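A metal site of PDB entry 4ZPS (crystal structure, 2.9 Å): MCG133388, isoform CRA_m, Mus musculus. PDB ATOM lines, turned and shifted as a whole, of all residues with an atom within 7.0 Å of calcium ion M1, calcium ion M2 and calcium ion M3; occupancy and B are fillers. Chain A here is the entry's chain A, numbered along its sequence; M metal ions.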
ATOM      1  N   ASN A 114      17.657  -4.760 -34.542  1.00  0.00           N
ATOM      2  CA  ASN A 114      17.850  -4.266 -33.185  1.00  0.00           C
ATOM      3  C   ASN A 114      16.713  -3.351 -32.764  1.00  0.00           C
ATOM      4  O   ASN A 114      16.104  -2.687 -33.594  1.00  0.00           O
ATOM      5  CB  ASN A 114      19.197  -3.536 -33.082  1.00  0.00           C
ATOM      6  CG  ASN A 114      19.625  -3.289 -31.648  1.00  0.00           C
ATOM      7  OD1 ASN A 114      18.817  -2.956 -30.785  1.00  0.00           O
ATOM      8  ND2 ASN A 114      20.913  -3.470 -31.385  1.00  0.00           N
ATOM      9  N   GLU A 115      16.426  -3.320 -31.459  1.00  0.00           N
ATOM     10  CA  GLU A 115      15.375  -2.470 -30.916  1.00  0.00           C
ATOM     11  C   GLU A 115      15.618  -0.995 -31.188  1.00  0.00           C
ATOM     12  O   GLU A 115      14.670  -0.226 -31.355  1.00  0.00           O
ATOM     13  CB  GLU A 115      15.252  -2.666 -29.402  1.00  0.00           C
ATOM     14  CG  GLU A 115      14.741  -4.005 -28.944  1.00  0.00           C
ATOM     15  CD  GLU A 115      14.696  -4.083 -27.447  1.00  0.00           C
ATOM     16  OE1 GLU A 115      15.599  -3.521 -26.795  1.00  0.00           O
ATOM     17  OE2 GLU A 115      13.751  -4.701 -26.906  1.00  0.00           O
ATOM     18  N   LEU A 171      10.437  -1.625 -32.390  1.00  0.00           N
ATOM     19  CA  LEU A 171      10.367  -2.964 -31.805  1.00  0.00           C
ATOM     20  C   LEU A 171      10.809  -2.935 -30.334  1.00  0.00           C
ATOM     21  O   LEU A 171      11.365  -1.940 -29.862  1.00  0.00           O
ATOM     22  CB  LEU A 171      11.232  -3.950 -32.598  1.00  0.00           C
ATOM     23  CG  LEU A 171      10.770  -4.226 -34.035  1.00  0.00           C
ATOM     24  CD1 LEU A 171      11.804  -5.048 -34.789  1.00  0.00           C
ATOM     25  CD2 LEU A 171       9.432  -4.939 -34.040  1.00  0.00           C
ATOM     26  N   ASP A 172      10.548  -4.034 -29.630  1.00  0.00           N
ATOM     27  CA  ASP A 172      10.910  -4.153 -28.221  1.00  0.00           C
ATOM     28  C   ASP A 172      10.929  -5.620 -27.806  1.00  0.00           C
ATOM     29  O   ASP A 172       9.879  -6.216 -27.564  1.00  0.00           O
ATOM     30  CB  ASP A 172       9.946  -3.357 -27.345  1.00  0.00           C
ATOM     31  CG  ASP A 172      10.309  -3.415 -25.868  1.00  0.00           C
ATOM     32  OD1 ASP A 172      11.502  -3.607 -25.550  1.00  0.00           O
ATOM     33  OD2 ASP A 172       9.393  -3.258 -25.032  1.00  0.00           O
ATOM     34  N   ARG A 173      12.124  -6.214 -27.713  1.00  0.00           N
ATOM     35  CA  ARG A 173      12.241  -7.630 -27.375  1.00  0.00           C
ATOM     36  C   ARG A 173      11.934  -7.888 -25.902  1.00  0.00           C
ATOM     37  O   ARG A 173      11.751  -9.025 -25.482  1.00  0.00           O
ATOM     38  CB  ARG A 173      13.627  -8.172 -27.728  1.00  0.00           C
ATOM     39  CG  ARG A 173      14.748  -7.652 -26.854  1.00  0.00           C
ATOM     40  CD  ARG A 173      15.836  -8.700 -26.654  1.00  0.00           C
ATOM     41  NE  ARG A 173      15.361  -9.823 -25.847  1.00  0.00           N
ATOM     42  CZ  ARG A 173      15.335  -9.828 -24.518  1.00  0.00           C
ATOM     43  NH1 ARG A 173      15.747  -8.767 -23.846  1.00  0.00           N
ATOM     44  NH2 ARG A 173      14.885 -10.892 -23.869  1.00  0.00           N
ATOM     45  N   GLU A 174      11.897  -6.820 -25.114  1.00  0.00           N
ATOM     46  CA  GLU A 174      11.496  -6.939 -23.714  1.00  0.00           C
ATOM     47  C   GLU A 174      10.010  -7.271 -23.632  1.00  0.00           C
ATOM     48  O   GLU A 174       9.527  -7.764 -22.609  1.00  0.00           O
ATOM     49  CB  GLU A 174      11.807  -5.654 -22.936  1.00  0.00           C
ATOM     50  CG  GLU A 174      13.245  -5.569 -22.443  1.00  0.00           C
ATOM     51  CD  GLU A 174      14.250  -5.313 -23.554  1.00  0.00           C
ATOM     52  OE1 GLU A 174      15.000  -6.241 -23.907  1.00  0.00           O
ATOM     53  OE2 GLU A 174      14.292  -4.172 -24.065  1.00  0.00           O
ATOM     54  N   GLU A 175       9.299  -7.015 -24.723  1.00  0.00           N
ATOM     55  CA  GLU A 175       7.890  -7.387 -24.843  1.00  0.00           C
ATOM     56  C   GLU A 175       7.714  -8.589 -25.766  1.00  0.00           C
ATOM     57  O   GLU A 175       7.045  -9.563 -25.412  1.00  0.00           O
ATOM     58  CB  GLU A 175       7.057  -6.202 -25.358  1.00  0.00           C
ATOM     59  CG  GLU A 175       6.723  -5.173 -24.302  1.00  0.00           C
ATOM     60  CD  GLU A 175       5.689  -5.676 -23.298  1.00  0.00           C
ATOM     61  OE1 GLU A 175       5.037  -6.700 -23.582  1.00  0.00           O
ATOM     62  OE2 GLU A 175       5.531  -5.041 -22.240  1.00  0.00           O
ATOM     63  N   LEU A 204      17.014  -8.276 -32.007  1.00  0.00           N
ATOM     64  CA  LEU A 204      18.234  -8.258 -31.216  1.00  0.00           C
ATOM     65  C   LEU A 204      18.090  -7.273 -30.064  1.00  0.00           C
ATOM     66  O   LEU A 204      17.240  -6.388 -30.099  1.00  0.00           O
ATOM     67  CB  LEU A 204      19.442  -7.906 -32.077  1.00  0.00           C
ATOM     68  CG  LEU A 204      19.649  -8.794 -33.303  1.00  0.00           C
ATOM     69  CD1 LEU A 204      20.957  -8.456 -34.017  1.00  0.00           C
ATOM     70  CD2 LEU A 204      19.607 -10.263 -32.929  1.00  0.00           C
ATOM     71  N   ASP A 205      18.920  -7.432 -29.036  1.00  0.00           N
ATOM     72  CA  ASP A 205      18.785  -6.628 -27.827  1.00  0.00           C
ATOM     73  C   ASP A 205      19.663  -5.388 -27.829  1.00  0.00           C
ATOM     74  O   ASP A 205      20.753  -5.383 -28.415  1.00  0.00           O
ATOM     75  CB  ASP A 205      19.119  -7.478 -26.595  1.00  0.00           C
ATOM     76  CG  ASP A 205      18.824  -6.752 -25.288  1.00  0.00           C
ATOM     77  OD1 ASP A 205      17.670  -6.797 -24.813  1.00  0.00           O
ATOM     78  OD2 ASP A 205      19.759  -6.136 -24.724  1.00  0.00           O
ATOM     79  N   THR A 206      19.174  -4.340 -27.185  1.00  0.00           N
ATOM     80  CA  THR A 206      19.990  -3.170 -26.851  1.00  0.00           C
ATOM     81  C   THR A 206      19.792  -2.875 -25.368  1.00  0.00           C
ATOM     82  O   THR A 206      18.755  -3.195 -24.796  1.00  0.00           O
ATOM     83  CB  THR A 206      19.612  -1.940 -27.699  1.00  0.00           C
ATOM     84  OG1 THR A 206      20.477  -0.842 -27.348  1.00  0.00           O
ATOM     85  CG2 THR A 206      18.165  -1.536 -27.453  1.00  0.00           C
ATOM     86  N   ASN A 207      20.807  -2.295 -24.743  1.00  0.00           N
ATOM     87  CA  ASN A 207      20.763  -2.034 -23.301  1.00  0.00           C
ATOM     88  C   ASN A 207      20.061  -0.709 -22.993  1.00  0.00           C
ATOM     89  O   ASN A 207      20.715   0.310 -22.759  1.00  0.00           O
ATOM     90  CB  ASN A 207      22.176  -2.037 -22.720  1.00  0.00           C
ATOM     91  CG  ASN A 207      22.185  -1.877 -21.221  1.00  0.00           C
ATOM     92  OD1 ASN A 207      21.889  -2.808 -20.479  1.00  0.00           O
ATOM     93  ND2 ASN A 207      22.538  -0.684 -20.759  1.00  0.00           N
ATOM     94  N   ASP A 208      18.735  -0.733 -22.988  1.00  0.00           N
ATOM     95  CA  ASP A 208      17.951   0.474 -22.774  1.00  0.00           C
ATOM     96  C   ASP A 208      17.211   0.450 -21.440  1.00  0.00           C
ATOM     97  O   ASP A 208      16.700   1.477 -20.984  1.00  0.00           O
ATOM     98  CB  ASP A 208      16.960   0.674 -23.921  1.00  0.00           C
ATOM     99  CG  ASP A 208      16.099  -0.546 -24.186  1.00  0.00           C
ATOM    100  OD1 ASP A 208      16.569  -1.680 -23.943  1.00  0.00           O
ATOM    101  OD2 ASP A 208      14.944  -0.382 -24.630  1.00  0.00           O
ATOM    102  N   ASN A 209      17.152  -0.716 -20.813  1.00  0.00           N
ATOM    103  CA  ASN A 209      16.549  -0.828 -19.485  1.00  0.00           C
ATOM    104  C   ASN A 209      17.568  -0.685 -18.367  1.00  0.00           C
ATOM    105  O   ASN A 209      18.437  -1.541 -18.195  1.00  0.00           O
ATOM    106  CB  ASN A 209      15.803  -2.160 -19.347  1.00  0.00           C
ATOM    107  CG  ASN A 209      14.494  -2.172 -20.095  1.00  0.00           C
ATOM    108  OD1 ASN A 209      14.372  -2.834 -21.130  1.00  0.00           O
ATOM    109  ND2 ASN A 209      13.503  -1.457 -19.585  1.00  0.00           N
ATOM    110  N   ALA A 210      17.469   0.403 -17.621  1.00  0.00           N
ATOM    111  CA  ALA A 210      18.320   0.627 -16.461  1.00  0.00           C
ATOM    112  C   ALA A 210      17.780  -0.139 -15.265  1.00  0.00           C
ATOM    113  O   ALA A 210      16.572  -0.339 -15.139  1.00  0.00           O
ATOM    114  CB  ALA A 210      18.414   2.113 -16.145  1.00  0.00           C
ATOM    115  N   PRO A 211      18.676  -0.598 -14.376  1.00  0.00           N
ATOM    116  CA  PRO A 211      18.290  -1.292 -13.145  1.00  0.00           C
ATOM    117  C   PRO A 211      17.328  -0.487 -12.280  1.00  0.00           C
ATOM    118  O   PRO A 211      17.561   0.698 -12.042  1.00  0.00           O
ATOM    119  CB  PRO A 211      19.627  -1.499 -12.423  1.00  0.00           C
ATOM    120  CG  PRO A 211      20.634  -1.535 -13.521  1.00  0.00           C
ATOM    121  CD  PRO A 211      20.139  -0.558 -14.553  1.00  0.00           C
ATOM    122  N   SER A 238      15.164  -4.886 -10.959  1.00  0.00           N
ATOM    123  CA  SER A 238      14.653  -5.448 -12.205  1.00  0.00           C
ATOM    124  C   SER A 238      15.426  -4.928 -13.424  1.00  0.00           C
ATOM    125  O   SER A 238      15.766  -3.753 -13.505  1.00  0.00           O
ATOM    126  CB  SER A 238      13.174  -5.127 -12.365  1.00  0.00           C
ATOM    127  OG  SER A 238      12.658  -5.662 -13.571  1.00  0.00           O
ATOM    128  N   ASP A 239      15.686  -5.830 -14.364  1.00  0.00           N
ATOM    129  CA  ASP A 239      16.360  -5.490 -15.611  1.00  0.00           C
ATOM    130  C   ASP A 239      16.028  -6.525 -16.670  1.00  0.00           C
ATOM    131  O   ASP A 239      16.665  -7.583 -16.728  1.00  0.00           O
ATOM    132  CB  ASP A 239      17.874  -5.397 -15.393  1.00  0.00           C
ATOM    133  CG  ASP A 239      18.562  -4.556 -16.442  1.00  0.00           C
ATOM    134  OD1 ASP A 239      18.114  -4.563 -17.610  1.00  0.00           O
ATOM    135  OD2 ASP A 239      19.558  -3.879 -16.102  1.00  0.00           O
ATOM    136  N   PRO A 240      15.034  -6.239 -17.518  1.00  0.00           N
ATOM    137  CA  PRO A 240      14.488  -7.182 -18.499  1.00  0.00           C
ATOM    138  C   PRO A 240      15.389  -7.392 -19.705  1.00  0.00           C
ATOM    139  O   PRO A 240      15.070  -8.218 -20.563  1.00  0.00           O
ATOM    140  CB  PRO A 240      13.169  -6.520 -18.930  1.00  0.00           C
ATOM    141  CG  PRO A 240      12.942  -5.381 -17.975  1.00  0.00           C
ATOM    142  CD  PRO A 240      14.293  -4.963 -17.525  1.00  0.00           C
ATOM    143  N   ASP A 241      16.499  -6.651 -19.780  1.00  0.00           N
ATOM    144  CA  ASP A 241      17.423  -6.775 -20.902  1.00  0.00           C
ATOM    145  C   ASP A 241      18.011  -8.184 -20.988  1.00  0.00           C
ATOM    146  O   ASP A 241      17.966  -8.943 -20.027  1.00  0.00           O
ATOM    147  CB  ASP A 241      18.538  -5.736 -20.788  1.00  0.00           C
ATOM    148  CG  ASP A 241      18.030  -4.320 -20.957  1.00  0.00           C
ATOM    149  OD1 ASP A 241      16.958  -4.141 -21.566  1.00  0.00           O
ATOM    150  OD2 ASP A 241      18.713  -3.386 -20.482  1.00  0.00           O
ATOM    151  N   GLU A 242      18.565  -8.511 -22.148  1.00  0.00           N
ATOM    152  CA  GLU A 242      19.006  -9.870 -22.427  1.00  0.00           C
ATOM    153  C   GLU A 242      20.414 -10.159 -21.903  1.00  0.00           C
ATOM    154  O   GLU A 242      21.346  -9.398 -22.155  1.00  0.00           O
ATOM    155  CB  GLU A 242      18.947 -10.151 -23.923  1.00  0.00           C
ATOM    156  CG  GLU A 242      19.301 -11.584 -24.308  1.00  0.00           C
ATOM    157  CD  GLU A 242      19.041 -11.859 -25.785  1.00  0.00           C
ATOM    158  OE1 GLU A 242      18.706 -10.904 -26.516  1.00  0.00           O
ATOM    159  OE2 GLU A 242      19.170 -13.033 -26.198  1.00  0.00           O
ATOM    160  N   VAL A 244      23.811 -10.387 -20.583  1.00  0.00           N
ATOM    161  CA  VAL A 244      24.802  -9.517 -19.968  1.00  0.00           C
ATOM    162  C   VAL A 244      24.208  -8.155 -19.616  1.00  0.00           C
ATOM    163  O   VAL A 244      24.543  -7.556 -18.589  1.00  0.00           O
ATOM    164  CB  VAL A 244      26.021  -9.328 -20.895  1.00  0.00           C
ATOM    165  CG1 VAL A 244      27.148  -8.650 -20.139  1.00  0.00           C
ATOM    166  CG2 VAL A 244      26.480 -10.668 -21.440  1.00  0.00           C
ATOM    167  N   ASN A 245      23.310  -7.659 -20.467  1.00  0.00           N
ATOM    168  CA  ASN A 245      22.650  -6.392 -20.243  1.00  0.00           C
ATOM    169  C   ASN A 245      21.611  -6.470 -19.115  1.00  0.00           C
ATOM    170  O   ASN A 245      21.084  -5.449 -18.677  1.00  0.00           O
ATOM    171  CB  ASN A 245      21.979  -5.899 -21.521  1.00  0.00           C
ATOM    172  CG  ASN A 245      22.964  -5.614 -22.630  1.00  0.00           C
ATOM    173  OD1 ASN A 245      24.051  -5.081 -22.398  1.00  0.00           O
ATOM    174  ND2 ASN A 245      22.594  -5.971 -23.855  1.00  0.00           N
ATOM    175  N   GLY A 246      21.334  -7.686 -18.667  1.00  0.00           N
ATOM    176  CA  GLY A 246      20.352  -7.892 -17.612  1.00  0.00           C
ATOM    177  C   GLY A 246      20.999  -8.295 -16.304  1.00  0.00           C
ATOM    178  O   GLY A 246      20.323  -8.409 -15.279  1.00  0.00           O
ATOM    179  N   LYS A 247      22.309  -8.515 -16.336  1.00  0.00           N
ATOM    180  CA  LYS A 247      23.056  -8.851 -15.136  1.00  0.00           C
ATOM    181  C   LYS A 247      23.146  -7.647 -14.211  1.00  0.00           C
ATOM    182  O   LYS A 247      23.756  -6.637 -14.547  1.00  0.00           O
ATOM    183  CB  LYS A 247      24.449  -9.352 -15.482  1.00  0.00           C
ATOM    184  CG  LYS A 247      25.291  -9.747 -14.283  1.00  0.00           C
ATOM    185  CD  LYS A 247      26.666 -10.247 -14.697  1.00  0.00           C
ATOM    186  CE  LYS A 247      27.534 -10.532 -13.477  1.00  0.00           C
ATOM    187  NZ  LYS A 247      28.878 -11.038 -13.855  1.00  0.00           N
ATOM    188  N   ASP A 294      24.356  -2.289 -14.077  1.00  0.00           N
ATOM    189  CA  ASP A 294      24.527  -3.256 -15.163  1.00  0.00           C
ATOM    190  C   ASP A 294      25.798  -2.933 -15.951  1.00  0.00           C
ATOM    191  O   ASP A 294      26.469  -1.939 -15.678  1.00  0.00           O
ATOM    192  CB  ASP A 294      23.314  -3.269 -16.086  1.00  0.00           C
ATOM    193  CG  ASP A 294      23.146  -1.974 -16.856  1.00  0.00           C
ATOM    194  OD1 ASP A 294      23.710  -0.944 -16.428  1.00  0.00           O
ATOM    195  OD2 ASP A 294      22.443  -1.984 -17.885  1.00  0.00           O
ATOM    196  N   VAL A 295      26.113  -3.764 -16.942  1.00  0.00           N
ATOM    197  CA  VAL A 295      27.343  -3.604 -17.697  1.00  0.00           C
ATOM    198  C   VAL A 295      27.367  -2.326 -18.526  1.00  0.00           C
ATOM    199  O   VAL A 295      28.433  -1.874 -18.955  1.00  0.00           O
ATOM    200  CB  VAL A 295      27.578  -4.809 -18.630  1.00  0.00           C
ATOM    201  CG1 VAL A 295      27.845  -6.063 -17.815  1.00  0.00           C
ATOM    202  CG2 VAL A 295      26.387  -5.004 -19.559  1.00  0.00           C
ATOM    203  N   GLY A 296      26.194  -1.744 -18.752  1.00  0.00           N
ATOM    204  CA  GLY A 296      26.109  -0.499 -19.482  1.00  0.00           C
ATOM    205  C   GLY A 296      26.286   0.711 -18.580  1.00  0.00           C
ATOM    206  O   GLY A 296      26.075   1.843 -19.003  1.00  0.00           O
ATOM    207  N   LEU A 298      24.473   1.656 -16.158  1.00  0.00           N
ATOM    208  CA  LEU A 298      23.212   2.298 -15.818  1.00  0.00           C
ATOM    209  C   LEU A 298      22.882   2.038 -14.352  1.00  0.00           C
ATOM    210  O   LEU A 298      22.984   0.912 -13.873  1.00  0.00           O
ATOM    211  CB  LEU A 298      22.078   1.803 -16.712  1.00  0.00           C
ATOM    212  CG  LEU A 298      22.236   1.975 -18.220  1.00  0.00           C
ATOM    213  CD1 LEU A 298      20.951   1.559 -18.923  1.00  0.00           C
ATOM    214  CD2 LEU A 298      22.608   3.400 -18.590  1.00  0.00           C
HETATM  215 CA    CA M   1      13.370  -2.167 -25.261  1.00  0.00          CA
HETATM  216 CA    CA M   2      16.707  -4.564 -24.353  1.00  0.00          CA
HETATM  217 CA    CA M   3      20.189  -3.168 -18.432  1.00  0.00          CA
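Calcium ion M3 is bound by the backbone carbonyl oxygen (O) of Asn 209 (2.4 Å).
O of Asn 245 is bound to calcium ion M3, at 2.5 Å.
Calcium ion M3 is bound by OD2 of Asp 239.
Calcium ion M3 is bound by OD2 of Asp 241 (2.5 Å).
Calcium ion M3 is bound by OD2 of Asp 294 (2.6 Å).
Calcium ion M3 is bound by OD1 of Asp 239, at 2.6 Å.
The side-chain amide oxygen (OD1) of Asn 207 is bound to calcium ion M3.
Calcium ion M3 has seven donor atoms within binding distance.
Calcium ion M1 is bound by OD1 of Asp 172, OD2 of Asp 208 and OE2 of Glu 174.
Slightly farther from calcium ion M1 lies OE1 of Glu 115 (3.0 Å).
Slightly farther from calcium ion M1 lies OE2 of Glu 115 (3.0 Å).
Of the 28 residues printed, 4 come within 4 Å of calcium ion M1.
Along chain A the residues within 4 Å of calcium ion M1 span positions 115 to 208.
The nearest printed residue that does not touch calcium ion M1 is Asn 209 (4.3 Å).
The side-chain carboxylate of Glu 174 sits close to the side-chain amide oxygen of Asn 209, 3.2 Å away.
The side-chain carboxylate of Glu 174 lies close to the guanidinium group of Arg 173.
The side-chain amide nitrogen (ND2) of Asn 245 lies within hydrogen-bond range of the side-chain carboxylate (OD2) of Asp 205 (3.0 Å).
NH1 of Arg 173 lies close to OD1 of Asp 205 (2.9 Å).
N of Glu 242 sits close to OD1 of Asp 205, 3.3 Å away.
The backbone NH of Leu 298 sits at hydrogen-bond distance from the side-chain carboxylate of Asp 294, at 2.7 Å.
The side-chain carboxylate of Asp 294 sits close to the backbone NH of Gly 296 (3.5 Å).
N of Glu 115 lies within hydrogen-bond range of O of Leu 204, at 3.5 Å.
Calcium ion M2 is bound by OE1 of Glu 174 (2.4 Å), OE2 of Glu 174 (2.5 Å), OD1 of Asp 205 (2.5 Å), O of Thr 206 (2.5 Å), OD1 of Asp 241 (2.8 Å) and OE1 of Glu 115 (2.9 Å).
Calcium ion M2 has six donor atoms within binding distance.
Slightly farther from calcium ion M2 lies the side-chain carboxylate (OD1) of Asp 208 (2.9 Å).
Six residues have an atom within 4 Å of calcium ion M3: Asn 207, Asn 209, Asp 239, Asp 241, Asn 245 and Asp 294.
The nearest printed residue that does not touch calcium ion M3 is Ala 210 (4.6 Å).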
